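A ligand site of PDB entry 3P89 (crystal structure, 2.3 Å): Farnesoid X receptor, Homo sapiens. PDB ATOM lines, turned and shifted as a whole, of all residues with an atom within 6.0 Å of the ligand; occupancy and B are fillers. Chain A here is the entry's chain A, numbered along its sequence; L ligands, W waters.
An oxygen (O3) of the ligand is in hydrogen-bond range of the side-chain hydroxyl (OG) of Ser 99 (2.8 Å). An oxygen (O4) of the ligand lies within salt-bridge range of the guanidinium group of Arg 88 (2.8 Å). N1 of the ligand sits at hydrogen-bond distance from NE2 of His 204 (3.0 Å).
The indole nitrogen of Trp 211 sits at hydrogen-bond distance from the backbone carbonyl oxygen of Ser 112 (2.8 Å). N of His 51 lies within hydrogen-bond range of SD of Met 22 (3.7 Å). The backbone carbonyl oxygen of Ile 92 lies within hydrogen-bond range of the backbone NH of Leu 97 (3.2 Å). OG of Ser 89 is in hydrogen-bond range of O of Phe 86 (2.9 Å). The side-chain hydroxyl (OG) of Ser 89 is in hydrogen-bond range of the side-chain hydroxyl (OH) of Tyr 126 (2.7 Å). OG1 of Thr 45 sits at hydrogen-bond distance from O of Phe 41. The side-chain hydroxyl (OG) of Ser 89 is in hydrogen-bond range of the backbone carbonyl oxygen (O) of Met 85 (2.9 Å). The side-chain hydroxyl (OG) of Ser 112 lies within hydrogen-bond range of the backbone carbonyl oxygen (O) of Ile 109 (3.0 Å).
Water W2 lies within hydrogen-bond range of O3 of the ligand (2.8 Å), OG1 of Thr 27 (2.8 Å) and O of Met 22 (2.9 Å). Water W1 lies within hydrogen-bond range of N2 of the ligand (2.8 Å) and NE of Arg 88 (3.0 Å).
CG of Met 22 touches N2 of the ligand (3.3 Å). CG2 of Thr 27 touches C19 of the ligand, at 3.3 Å. Phe 41 touches the ligand (CE1 to C3, 3.5 Å). Leu 44 touches the ligand (O to C7, 3.6 Å). Thr 45 touches the ligand. Met 47 touches the ligand (CB to C11, 3.96 Å). Ala 48 touches the ligand. His 51 touches the ligand. SD of Met 85 touches CL2 of the ligand, 3.6 Å away. Phe 86 touches the ligand (CD1 to C28, 3.4 Å). Ser 89 touches the ligand. Ile 92 touches the ligand. Leu 97 touches the ligand (CD2 to O3, 3.4 Å). Gly 100 touches the ligand. Ile 109 touches the ligand. Ile 114 touches the ligand. Met 122 touches the ligand. Tyr 126 touches the ligand. CZ3 of Trp 211 touches O1 of the ligand, at 3.2 Å. CD2 of Phe 218 touches C1 of the ligand (3.9 Å). Trp 226 touches the ligand. Hydrophobic or aromatic side chains within 4 Å of the ligand: Met 22, Phe 41, Leu 44, Met 47, Ala 48, His 51, Met 85, Phe 86, Ile 92, Leu 97, Ile 109, Ile 114, Met 122, His 204, Trp 211, Phe 218 and Trp 226. Of the 33 residues printed, 24 come within 4 Å of the ligand.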
ATOM      1  N   ARG A  21     -17.148 -11.275  12.192  1.00  0.00           N
ATOM      2  CA  ARG A  21     -16.623 -11.694  10.887  1.00  0.00           C
ATOM      3  C   ARG A  21     -17.097 -10.760   9.769  1.00  0.00           C
ATOM      4  O   ARG A  21     -18.200 -10.211   9.816  1.00  0.00           O
ATOM      5  CB  ARG A  21     -17.049 -13.120  10.590  1.00  0.00           C
ATOM      6  N   MET A  22     -16.244 -10.605   8.755  1.00  0.00           N
ATOM      7  CA  MET A  22     -16.550  -9.791   7.590  1.00  0.00           C
ATOM      8  C   MET A  22     -17.550 -10.546   6.719  1.00  0.00           C
ATOM      9  O   MET A  22     -17.325 -11.702   6.385  1.00  0.00           O
ATOM     10  CB  MET A  22     -15.288  -9.546   6.780  1.00  0.00           C
ATOM     11  CG  MET A  22     -14.185  -8.835   7.544  1.00  0.00           C
ATOM     12  SD  MET A  22     -14.375  -7.050   7.622  1.00  0.00           S
ATOM     13  CE  MET A  22     -14.162  -6.621   5.895  1.00  0.00           C
ATOM     14  N   THR A  27     -16.474  -8.983   1.257  1.00  0.00           N
ATOM     15  CA  THR A  27     -15.143  -9.467   0.865  1.00  0.00           C
ATOM     16  C   THR A  27     -15.094 -10.021  -0.571  1.00  0.00           C
ATOM     17  O   THR A  27     -14.016 -10.046  -1.173  1.00  0.00           O
ATOM     18  CB  THR A  27     -14.617 -10.533   1.845  1.00  0.00           C
ATOM     19  OG1 THR A  27     -15.561 -11.606   1.955  1.00  0.00           O
ATOM     20  CG2 THR A  27     -14.378  -9.925   3.208  1.00  0.00           C
ATOM     21  N   ILE A  30     -13.301  -7.901  -3.366  1.00  0.00           N
ATOM     22  CA  ILE A  30     -11.859  -8.012  -3.593  1.00  0.00           C
ATOM     23  C   ILE A  30     -11.603  -8.761  -4.896  1.00  0.00           C
ATOM     24  O   ILE A  30     -10.759  -8.355  -5.708  1.00  0.00           O
ATOM     25  CB  ILE A  30     -11.136  -8.732  -2.407  1.00  0.00           C
ATOM     26  CG1 ILE A  30     -11.262  -7.917  -1.108  1.00  0.00           C
ATOM     27  CG2 ILE A  30      -9.657  -8.932  -2.722  1.00  0.00           C
ATOM     28  CD1 ILE A  30     -11.058  -8.758   0.167  1.00  0.00           C
ATOM     29  N   PHE A  41      -8.593   1.438  -4.178  1.00  0.00           N
ATOM     30  CA  PHE A  41      -8.671   2.283  -2.993  1.00  0.00           C
ATOM     31  C   PHE A  41     -10.036   2.200  -2.298  1.00  0.00           C
ATOM     32  O   PHE A  41     -10.105   2.070  -1.075  1.00  0.00           O
ATOM     33  CB  PHE A  41      -8.361   3.749  -3.342  1.00  0.00           C
ATOM     34  CG  PHE A  41      -8.461   4.670  -2.170  1.00  0.00           C
ATOM     35  CD1 PHE A  41      -7.374   4.854  -1.335  1.00  0.00           C
ATOM     36  CD2 PHE A  41      -9.660   5.317  -1.883  1.00  0.00           C
ATOM     37  CE1 PHE A  41      -7.472   5.687  -0.233  1.00  0.00           C
ATOM     38  CE2 PHE A  41      -9.767   6.151  -0.792  1.00  0.00           C
ATOM     39  CZ  PHE A  41      -8.667   6.330   0.041  1.00  0.00           C
ATOM     40  N   LEU A  44     -10.386  -1.242  -0.519  1.00  0.00           N
ATOM     41  CA  LEU A  44      -9.561  -1.242   0.695  1.00  0.00           C
ATOM     42  C   LEU A  44     -10.173  -0.400   1.822  1.00  0.00           C
ATOM     43  O   LEU A  44     -10.145  -0.790   2.988  1.00  0.00           O
ATOM     44  CB  LEU A  44      -8.145  -0.739   0.365  1.00  0.00           C
ATOM     45  CG  LEU A  44      -7.330  -1.660  -0.548  1.00  0.00           C
ATOM     46  CD1 LEU A  44      -5.994  -1.033  -0.899  1.00  0.00           C
ATOM     47  CD2 LEU A  44      -7.129  -3.034   0.079  1.00  0.00           C
ATOM     48  N   THR A  45     -10.714   0.774   1.473  1.00  0.00           N
ATOM     49  CA  THR A  45     -11.394   1.637   2.440  1.00  0.00           C
ATOM     50  C   THR A  45     -12.613   0.935   3.051  1.00  0.00           C
ATOM     51  O   THR A  45     -12.827   0.991   4.263  1.00  0.00           O
ATOM     52  CB  THR A  45     -11.846   2.972   1.796  1.00  0.00           C
ATOM     53  OG1 THR A  45     -10.697   3.693   1.327  1.00  0.00           O
ATOM     54  CG2 THR A  45     -12.600   3.837   2.800  1.00  0.00           C
ATOM     55  N   MET A  47     -13.114  -2.365   3.223  1.00  0.00           N
ATOM     56  CA  MET A  47     -12.591  -3.462   4.071  1.00  0.00           C
ATOM     57  C   MET A  47     -12.143  -2.924   5.423  1.00  0.00           C
ATOM     58  O   MET A  47     -12.505  -3.483   6.462  1.00  0.00           O
ATOM     59  CB  MET A  47     -11.421  -4.178   3.393  1.00  0.00           C
ATOM     60  CG  MET A  47     -11.727  -4.815   2.034  1.00  0.00           C
ATOM     61  SD  MET A  47     -13.196  -5.864   2.054  1.00  0.00           S
ATOM     62  CE  MET A  47     -14.109  -5.178   0.664  1.00  0.00           C
ATOM     63  N   ALA A  48     -11.389  -1.827   5.404  1.00  0.00           N
ATOM     64  CA  ALA A  48     -10.855  -1.207   6.635  1.00  0.00           C
ATOM     65  C   ALA A  48     -11.962  -0.720   7.559  1.00  0.00           C
ATOM     66  O   ALA A  48     -11.927  -0.962   8.766  1.00  0.00           O
ATOM     67  CB  ALA A  48      -9.920  -0.051   6.298  1.00  0.00           C
ATOM     68  N   HIS A  51     -13.687  -3.666   8.992  1.00  0.00           N
ATOM     69  CA  HIS A  51     -12.815  -4.334   9.962  1.00  0.00           C
ATOM     70  C   HIS A  51     -12.720  -3.586  11.285  1.00  0.00           C
ATOM     71  O   HIS A  51     -12.599  -4.215  12.337  1.00  0.00           O
ATOM     72  CB  HIS A  51     -11.411  -4.558   9.392  1.00  0.00           C
ATOM     73  CG  HIS A  51     -10.522  -5.319  10.325  1.00  0.00           C
ATOM     74  ND1 HIS A  51     -10.881  -6.537  10.871  1.00  0.00           N
ATOM     75  CD2 HIS A  51      -9.293  -5.034  10.811  1.00  0.00           C
ATOM     76  CE1 HIS A  51      -9.916  -6.968  11.655  1.00  0.00           C
ATOM     77  NE2 HIS A  51      -8.934  -6.075  11.636  1.00  0.00           N
ATOM     78  N   ALA A  81      -5.362   0.452  16.160  1.00  0.00           N
ATOM     79  CA  ALA A  81      -6.164   0.239  14.957  1.00  0.00           C
ATOM     80  C   ALA A  81      -5.317  -0.200  13.781  1.00  0.00           C
ATOM     81  O   ALA A  81      -5.535  -1.253  13.211  1.00  0.00           O
ATOM     82  CB  ALA A  81      -6.950   1.508  14.605  1.00  0.00           C
ATOM     83  N   VAL A  82      -4.319   0.611  13.424  1.00  0.00           N
ATOM     84  CA  VAL A  82      -3.444   0.310  12.307  1.00  0.00           C
ATOM     85  C   VAL A  82      -2.734  -1.030  12.525  1.00  0.00           C
ATOM     86  O   VAL A  82      -2.717  -1.883  11.625  1.00  0.00           O
ATOM     87  CB  VAL A  82      -2.405   1.431  12.084  1.00  0.00           C
ATOM     88  CG1 VAL A  82      -1.391   1.031  11.014  1.00  0.00           C
ATOM     89  CG2 VAL A  82      -3.101   2.734  11.711  1.00  0.00           C
ATOM     90  N   MET A  85      -4.967  -4.043  12.091  1.00  0.00           N
ATOM     91  CA  MET A  85      -5.299  -4.271  10.683  1.00  0.00           C
ATOM     92  C   MET A  85      -4.138  -4.901   9.922  1.00  0.00           C
ATOM     93  O   MET A  85      -4.346  -5.763   9.075  1.00  0.00           O
ATOM     94  CB  MET A  85      -5.704  -2.976   9.984  1.00  0.00           C
ATOM     95  CG  MET A  85      -6.940  -2.320  10.565  1.00  0.00           C
ATOM     96  SD  MET A  85      -7.527  -0.866   9.677  1.00  0.00           S
ATOM     97  CE  MET A  85      -8.333   0.002  11.004  1.00  0.00           C
ATOM     98  N   PHE A  86      -2.924  -4.449  10.227  1.00  0.00           N
ATOM     99  CA  PHE A  86      -1.722  -5.085   9.673  1.00  0.00           C
ATOM    100  C   PHE A  86      -1.637  -6.548  10.079  1.00  0.00           C
ATOM    101  O   PHE A  86      -1.317  -7.403   9.270  1.00  0.00           O
ATOM    102  CB  PHE A  86      -0.442  -4.351  10.092  1.00  0.00           C
ATOM    103  CG  PHE A  86      -0.005  -3.303   9.111  1.00  0.00           C
ATOM    104  CD1 PHE A  86      -0.467  -1.999   9.226  1.00  0.00           C
ATOM    105  CD2 PHE A  86       0.832  -3.632   8.056  1.00  0.00           C
ATOM    106  CE1 PHE A  86      -0.073  -1.026   8.308  1.00  0.00           C
ATOM    107  CE2 PHE A  86       1.229  -2.668   7.135  1.00  0.00           C
ATOM    108  CZ  PHE A  86       0.776  -1.365   7.261  1.00  0.00           C
ATOM    109  N   ARG A  88      -4.155  -8.633  11.108  1.00  0.00           N
ATOM    110  CA  ARG A  88      -5.223  -9.400  10.465  1.00  0.00           C
ATOM    111  C   ARG A  88      -4.963  -9.602   8.967  1.00  0.00           C
ATOM    112  O   ARG A  88      -5.178 -10.695   8.447  1.00  0.00           O
ATOM    113  CB  ARG A  88      -6.580  -8.727  10.695  1.00  0.00           C
ATOM    114  CG  ARG A  88      -7.773  -9.414  10.010  1.00  0.00           C
ATOM    115  CD  ARG A  88      -7.935 -10.863  10.444  1.00  0.00           C
ATOM    116  NE  ARG A  88      -9.107 -11.478   9.802  1.00  0.00           N
ATOM    117  CZ  ARG A  88      -9.435 -12.765   9.875  1.00  0.00           C
ATOM    118  NH1 ARG A  88      -8.689 -13.620  10.571  1.00  0.00           N
ATOM    119  NH2 ARG A  88     -10.519 -13.201   9.250  1.00  0.00           N
ATOM    120  N   SER A  89      -4.494  -8.564   8.290  1.00  0.00           N
ATOM    121  CA  SER A  89      -4.141  -8.681   6.879  1.00  0.00           C
ATOM    122  C   SER A  89      -2.956  -9.645   6.687  1.00  0.00           C
ATOM    123  O   SER A  89      -2.919 -10.419   5.724  1.00  0.00           O
ATOM    124  CB  SER A  89      -3.855  -7.311   6.249  1.00  0.00           C
ATOM    125  OG  SER A  89      -2.749  -6.661   6.846  1.00  0.00           O
ATOM    126  N   ILE A  92      -4.330 -13.089   6.744  1.00  0.00           N
ATOM    127  CA  ILE A  92      -4.965 -13.435   5.468  1.00  0.00           C
ATOM    128  C   ILE A  92      -3.937 -13.926   4.470  1.00  0.00           C
ATOM    129  O   ILE A  92      -4.074 -15.013   3.926  1.00  0.00           O
ATOM    130  CB  ILE A  92      -5.741 -12.233   4.882  1.00  0.00           C
ATOM    131  CG1 ILE A  92      -6.986 -11.949   5.709  1.00  0.00           C
ATOM    132  CG2 ILE A  92      -6.126 -12.500   3.431  1.00  0.00           C
ATOM    133  CD1 ILE A  92      -7.543 -10.575   5.475  1.00  0.00           C
ATOM    134  N   LEU A  97      -6.430 -17.198   3.655  1.00  0.00           N
ATOM    135  CA  LEU A  97      -7.859 -17.291   3.981  1.00  0.00           C
ATOM    136  C   LEU A  97      -8.665 -17.106   2.694  1.00  0.00           C
ATOM    137  O   LEU A  97      -8.533 -16.094   2.021  1.00  0.00           O
ATOM    138  CB  LEU A  97      -8.265 -16.221   5.004  1.00  0.00           C
ATOM    139  CG  LEU A  97      -9.732 -16.230   5.427  1.00  0.00           C
ATOM    140  CD1 LEU A  97     -10.056 -17.480   6.246  1.00  0.00           C
ATOM    141  CD2 LEU A  97     -10.104 -14.959   6.200  1.00  0.00           C
ATOM    142  N   SER A  99     -11.769 -16.341   1.854  1.00  0.00           N
ATOM    143  CA  SER A  99     -12.547 -15.119   1.723  1.00  0.00           C
ATOM    144  C   SER A  99     -11.711 -13.845   1.753  1.00  0.00           C
ATOM    145  O   SER A  99     -12.237 -12.761   1.563  1.00  0.00           O
ATOM    146  CB  SER A  99     -13.656 -15.066   2.758  1.00  0.00           C
ATOM    147  OG  SER A  99     -13.203 -15.534   4.016  1.00  0.00           O
ATOM    148  N   GLY A 100     -10.415 -13.972   2.008  1.00  0.00           N
ATOM    149  CA  GLY A 100      -9.478 -12.853   1.861  1.00  0.00           C
ATOM    150  C   GLY A 100      -8.988 -12.621   0.435  1.00  0.00           C
ATOM    151  O   GLY A 100      -8.521 -11.527   0.118  1.00  0.00           O
ATOM    152  N   LEU A 105      -6.281  -9.319  -3.266  1.00  0.00           N
ATOM    153  CA  LEU A 105      -6.096  -8.286  -2.229  1.00  0.00           C
ATOM    154  C   LEU A 105      -4.733  -7.615  -2.428  1.00  0.00           C
ATOM    155  O   LEU A 105      -4.619  -6.382  -2.380  1.00  0.00           O
ATOM    156  CB  LEU A 105      -6.191  -8.883  -0.834  1.00  0.00           C
ATOM    157  CG  LEU A 105      -6.105  -7.915   0.351  1.00  0.00           C
ATOM    158  CD1 LEU A 105      -7.277  -6.931   0.358  1.00  0.00           C
ATOM    159  CD2 LEU A 105      -6.073  -8.681   1.665  1.00  0.00           C
ATOM    160  N   ILE A 109      -3.789  -3.632  -3.124  1.00  0.00           N
ATOM    161  CA  ILE A 109      -2.884  -2.879  -2.262  1.00  0.00           C
ATOM    162  C   ILE A 109      -1.737  -2.282  -3.066  1.00  0.00           C
ATOM    163  O   ILE A 109      -1.356  -1.136  -2.835  1.00  0.00           O
ATOM    164  CB  ILE A 109      -2.312  -3.741  -1.106  1.00  0.00           C
ATOM    165  CG1 ILE A 109      -3.439  -4.169  -0.153  1.00  0.00           C
ATOM    166  CG2 ILE A 109      -1.260  -2.966  -0.352  1.00  0.00           C
ATOM    167  CD1 ILE A 109      -3.011  -5.172   0.888  1.00  0.00           C
ATOM    168  N   SER A 112      -3.088   1.197  -5.271  1.00  0.00           N
ATOM    169  CA  SER A 112      -4.071   2.014  -4.567  1.00  0.00           C
ATOM    170  C   SER A 112      -3.512   3.385  -4.162  1.00  0.00           C
ATOM    171  O   SER A 112      -4.093   4.059  -3.310  1.00  0.00           O
ATOM    172  CB  SER A 112      -4.561   1.277  -3.320  1.00  0.00           C
ATOM    173  OG  SER A 112      -3.478   0.989  -2.454  1.00  0.00           O
ATOM    174  N   ILE A 114      -0.312   3.874  -2.929  1.00  0.00           N
ATOM    175  CA  ILE A 114       0.688   3.740  -1.865  1.00  0.00           C
ATOM    176  C   ILE A 114       2.096   3.807  -2.444  1.00  0.00           C
ATOM    177  O   ILE A 114       2.375   3.188  -3.462  1.00  0.00           O
ATOM    178  CB  ILE A 114       0.529   2.428  -1.069  1.00  0.00           C
ATOM    179  CG1 ILE A 114      -0.873   2.303  -0.482  1.00  0.00           C
ATOM    180  CG2 ILE A 114       1.563   2.373   0.063  1.00  0.00           C
ATOM    181  CD1 ILE A 114      -1.131   0.955   0.182  1.00  0.00           C
ATOM    182  N   MET A 122       5.930  -3.313   4.019  1.00  0.00           N
ATOM    183  CA  MET A 122       4.630  -3.929   4.290  1.00  0.00           C
ATOM    184  C   MET A 122       4.681  -5.409   3.957  1.00  0.00           C
ATOM    185  O   MET A 122       4.333  -6.258   4.779  1.00  0.00           O
ATOM    186  CB  MET A 122       3.512  -3.225   3.499  1.00  0.00           C
ATOM    187  CG  MET A 122       2.140  -3.915   3.526  1.00  0.00           C
ATOM    188  SD  MET A 122       0.836  -3.051   2.567  1.00  0.00           S
ATOM    189  CE  MET A 122       1.084  -1.344   3.109  1.00  0.00           C
ATOM    190  N   TYR A 126       4.831  -8.985   6.050  1.00  0.00           N
ATOM    191  CA  TYR A 126       3.902 -10.107   5.826  1.00  0.00           C
ATOM    192  C   TYR A 126       4.647 -11.437   5.637  1.00  0.00           C
ATOM    193  O   TYR A 126       4.212 -12.466   6.147  1.00  0.00           O
ATOM    194  CB  TYR A 126       3.038  -9.872   4.587  1.00  0.00           C
ATOM    195  CG  TYR A 126       1.979  -8.781   4.703  1.00  0.00           C
ATOM    196  CD1 TYR A 126       1.269  -8.596   5.882  1.00  0.00           C
ATOM    197  CD2 TYR A 126       1.679  -7.970   3.613  1.00  0.00           C
ATOM    198  CE1 TYR A 126       0.296  -7.622   5.978  1.00  0.00           C
ATOM    199  CE2 TYR A 126       0.699  -6.975   3.706  1.00  0.00           C
ATOM    200  CZ  TYR A 126       0.007  -6.821   4.896  1.00  0.00           C
ATOM    201  OH  TYR A 126      -0.968  -5.855   5.010  1.00  0.00           O
ATOM    202  N   HIS A 204       1.835   4.598   7.927  1.00  0.00           N
ATOM    203  CA  HIS A 204       0.408   4.811   7.697  1.00  0.00           C
ATOM    204  C   HIS A 204      -0.010   6.273   7.773  1.00  0.00           C
ATOM    205  O   HIS A 204      -0.852   6.722   6.985  1.00  0.00           O
ATOM    206  CB  HIS A 204      -0.448   3.976   8.654  1.00  0.00           C
ATOM    207  CG  HIS A 204      -1.862   3.809   8.201  1.00  0.00           C
ATOM    208  ND1 HIS A 204      -2.899   4.564   8.710  1.00  0.00           N
ATOM    209  CD2 HIS A 204      -2.401   3.006   7.263  1.00  0.00           C
ATOM    210  CE1 HIS A 204      -4.024   4.207   8.104  1.00  0.00           C
ATOM    211  NE2 HIS A 204      -3.747   3.270   7.224  1.00  0.00           N
ATOM    212  N   MET A 207       0.999   7.657   4.557  1.00  0.00           N
ATOM    213  CA  MET A 207       0.116   7.157   3.510  1.00  0.00           C
ATOM    214  C   MET A 207      -1.174   7.969   3.477  1.00  0.00           C
ATOM    215  O   MET A 207      -1.634   8.359   2.415  1.00  0.00           O
ATOM    216  CB  MET A 207      -0.196   5.664   3.716  1.00  0.00           C
ATOM    217  CG  MET A 207       1.016   4.727   3.602  1.00  0.00           C
ATOM    218  SD  MET A 207       0.629   3.012   4.036  1.00  0.00           S
ATOM    219  CE  MET A 207       2.036   2.523   4.997  1.00  0.00           C
ATOM    220  N   LEU A 208      -1.746   8.219   4.664  1.00  0.00           N
ATOM    221  CA  LEU A 208      -2.958   9.017   4.785  1.00  0.00           C
ATOM    222  C   LEU A 208      -2.750  10.434   4.244  1.00  0.00           C
ATOM    223  O   LEU A 208      -3.614  10.954   3.549  1.00  0.00           O
ATOM    224  CB  LEU A 208      -3.426   9.091   6.244  1.00  0.00           C
ATOM    225  CG  LEU A 208      -4.014   7.828   6.871  1.00  0.00           C
ATOM    226  CD1 LEU A 208      -4.539   8.159   8.258  1.00  0.00           C
ATOM    227  CD2 LEU A 208      -5.125   7.243   6.007  1.00  0.00           C
ATOM    228  N   TRP A 211      -2.655  10.280   0.380  1.00  0.00           N
ATOM    229  CA  TRP A 211      -4.021  10.050  -0.096  1.00  0.00           C
ATOM    230  C   TRP A 211      -4.886  11.299   0.026  1.00  0.00           C
ATOM    231  O   TRP A 211      -5.674  11.596  -0.875  1.00  0.00           O
ATOM    232  CB  TRP A 211      -4.678   8.900   0.671  1.00  0.00           C
ATOM    233  CG  TRP A 211      -4.328   7.533   0.182  1.00  0.00           C
ATOM    234  CD1 TRP A 211      -4.157   7.136  -1.111  1.00  0.00           C
ATOM    235  CD2 TRP A 211      -4.147   6.358   0.989  1.00  0.00           C
ATOM    236  NE1 TRP A 211      -3.870   5.793  -1.160  1.00  0.00           N
ATOM    237  CE2 TRP A 211      -3.850   5.291   0.110  1.00  0.00           C
ATOM    238  CE3 TRP A 211      -4.200   6.105   2.369  1.00  0.00           C
ATOM    239  CZ2 TRP A 211      -3.607   3.999   0.569  1.00  0.00           C
ATOM    240  CZ3 TRP A 211      -3.965   4.814   2.816  1.00  0.00           C
ATOM    241  CH2 TRP A 211      -3.664   3.779   1.919  1.00  0.00           C
ATOM    242  N   PHE A 218     -12.062   9.219   3.373  1.00  0.00           N
ATOM    243  CA  PHE A 218     -12.235   7.944   4.031  1.00  0.00           C
ATOM    244  C   PHE A 218     -13.665   7.858   4.546  1.00  0.00           C
ATOM    245  O   PHE A 218     -14.535   8.520   4.008  1.00  0.00           O
ATOM    246  CB  PHE A 218     -11.154   7.812   5.114  1.00  0.00           C
ATOM    247  CG  PHE A 218      -9.764   7.919   4.561  1.00  0.00           C
ATOM    248  CD1 PHE A 218      -9.101   9.130   4.539  1.00  0.00           C
ATOM    249  CD2 PHE A 218      -9.150   6.816   4.000  1.00  0.00           C
ATOM    250  CE1 PHE A 218      -7.820   9.234   3.997  1.00  0.00           C
ATOM    251  CE2 PHE A 218      -7.875   6.908   3.452  1.00  0.00           C
ATOM    252  CZ  PHE A 218      -7.207   8.123   3.454  1.00  0.00           C
ATOM    253  N   LEU A 222     -13.380   5.550  10.151  1.00  0.00           N
ATOM    254  CA  LEU A 222     -11.931   5.586   9.966  1.00  0.00           C
ATOM    255  C   LEU A 222     -11.380   6.973  10.290  1.00  0.00           C
ATOM    256  O   LEU A 222     -10.334   7.093  10.921  1.00  0.00           O
ATOM    257  CB  LEU A 222     -11.547   5.194   8.529  1.00  0.00           C
ATOM    258  CG  LEU A 222     -11.856   3.759   8.108  1.00  0.00           C
ATOM    259  CD1 LEU A 222     -11.570   3.546   6.607  1.00  0.00           C
ATOM    260  CD2 LEU A 222     -11.078   2.764   8.965  1.00  0.00           C
ATOM    261  N   TRP A 226      -8.549   7.214  13.149  1.00  0.00           N
ATOM    262  CA  TRP A 226      -7.222   7.655  12.677  1.00  0.00           C
ATOM    263  C   TRP A 226      -6.978   9.162  12.807  1.00  0.00           C
ATOM    264  O   TRP A 226      -5.916   9.636  12.413  1.00  0.00           O
ATOM    265  CB  TRP A 226      -7.010   7.246  11.218  1.00  0.00           C
ATOM    266  CG  TRP A 226      -6.872   5.765  10.979  1.00  0.00           C
ATOM    267  CD1 TRP A 226      -6.450   4.817  11.869  1.00  0.00           C
ATOM    268  CD2 TRP A 226      -7.125   5.078   9.745  1.00  0.00           C
ATOM    269  NE1 TRP A 226      -6.450   3.577  11.273  1.00  0.00           N
ATOM    270  CE2 TRP A 226      -6.860   3.710   9.978  1.00  0.00           C
ATOM    271  CE3 TRP A 226      -7.553   5.482   8.474  1.00  0.00           C
ATOM    272  CZ2 TRP A 226      -6.998   2.742   8.973  1.00  0.00           C
ATOM    273  CZ3 TRP A 226      -7.695   4.519   7.481  1.00  0.00           C
ATOM    274  CH2 TRP A 226      -7.420   3.166   7.743  1.00  0.00           C
HETATM  275  C1  LIG L   1      -8.312   2.992   4.188  1.00  0.00           C
HETATM  276  C2  LIG L   1      -7.647   2.092   3.151  1.00  0.00           C
HETATM  277  C3  LIG L   1      -7.317   2.844   1.874  1.00  0.00           C
HETATM  278  C4  LIG L   1      -6.426   1.524   3.758  1.00  0.00           C
HETATM  279  O1  LIG L   1      -5.443   2.363   4.151  1.00  0.00           O
HETATM  280  N1  LIG L   1      -4.312   1.669   4.720  1.00  0.00           N
HETATM  281  C5  LIG L   1      -4.605   0.343   4.693  1.00  0.00           C
HETATM  282  C6  LIG L   1      -5.959   0.170   4.079  1.00  0.00           C
HETATM  283  C7  LIG L   1      -6.709  -1.122   3.832  1.00  0.00           C
HETATM  284  O2  LIG L   1      -6.607  -1.907   5.002  1.00  0.00           O
HETATM  285  C8  LIG L   1      -7.211  -3.115   5.139  1.00  0.00           C
HETATM  286  C9  LIG L   1      -7.898  -3.333   6.316  1.00  0.00           C
HETATM  287  C10 LIG L   1      -8.524  -4.540   6.549  1.00  0.00           C
HETATM  288  C11 LIG L   1      -8.465  -5.575   5.631  1.00  0.00           C
HETATM  289  C12 LIG L   1      -7.774  -5.359   4.433  1.00  0.00           C
HETATM  290  C13 LIG L   1      -7.132  -4.133   4.197  1.00  0.00           C
HETATM  291  C14 LIG L   1      -9.195  -6.839   5.930  1.00  0.00           C
HETATM  292  C15 LIG L   1      -9.507  -7.157   7.260  1.00  0.00           C
HETATM  293  C16 LIG L   1     -10.211  -8.309   7.564  1.00  0.00           C
HETATM  294  C17 LIG L   1     -10.622  -9.157   6.553  1.00  0.00           C
HETATM  295  N2  LIG L   1     -11.308 -10.274   6.874  1.00  0.00           N
HETATM  296  C18 LIG L   1     -11.731 -11.124   5.915  1.00  0.00           C
HETATM  297  C19 LIG L   1     -11.467 -10.876   4.563  1.00  0.00           C
HETATM  298  C20 LIG L   1     -10.766  -9.720   4.216  1.00  0.00           C
HETATM  299  C21 LIG L   1     -10.335  -8.858   5.213  1.00  0.00           C
HETATM  300  C22 LIG L   1      -9.626  -7.694   4.914  1.00  0.00           C
HETATM  301  C23 LIG L   1     -12.496 -12.341   6.351  1.00  0.00           C
HETATM  302  O3  LIG L   1     -12.909 -13.169   5.554  1.00  0.00           O
HETATM  303  O4  LIG L   1     -12.757 -12.467   7.657  1.00  0.00           O
HETATM  304  C24 LIG L   1      -3.775  -0.789   5.183  1.00  0.00           C
HETATM  305  C25 LIG L   1      -3.098  -1.585   4.277  1.00  0.00           C
HETATM  306 CL1  LIG L   1      -3.204  -1.192   2.540  1.00  0.00          CL
HETATM  307  C26 LIG L   1      -2.332  -2.657   4.721  1.00  0.00           C
HETATM  308  C27 LIG L   1      -2.263  -2.945   6.085  1.00  0.00           C
HETATM  309  C28 LIG L   1      -2.959  -2.154   6.987  1.00  0.00           C
HETATM  310  C29 LIG L   1      -3.711  -1.085   6.533  1.00  0.00           C
HETATM  311 CL2  LIG L   1      -4.583  -0.067   7.700  1.00  0.00          CL
HETATM  312  O   HOH W   1     -11.944 -10.388   9.599  1.00  0.00           O
HETATM  313  O   HOH W   2     -15.421 -12.717   4.493  1.00  0.00           O
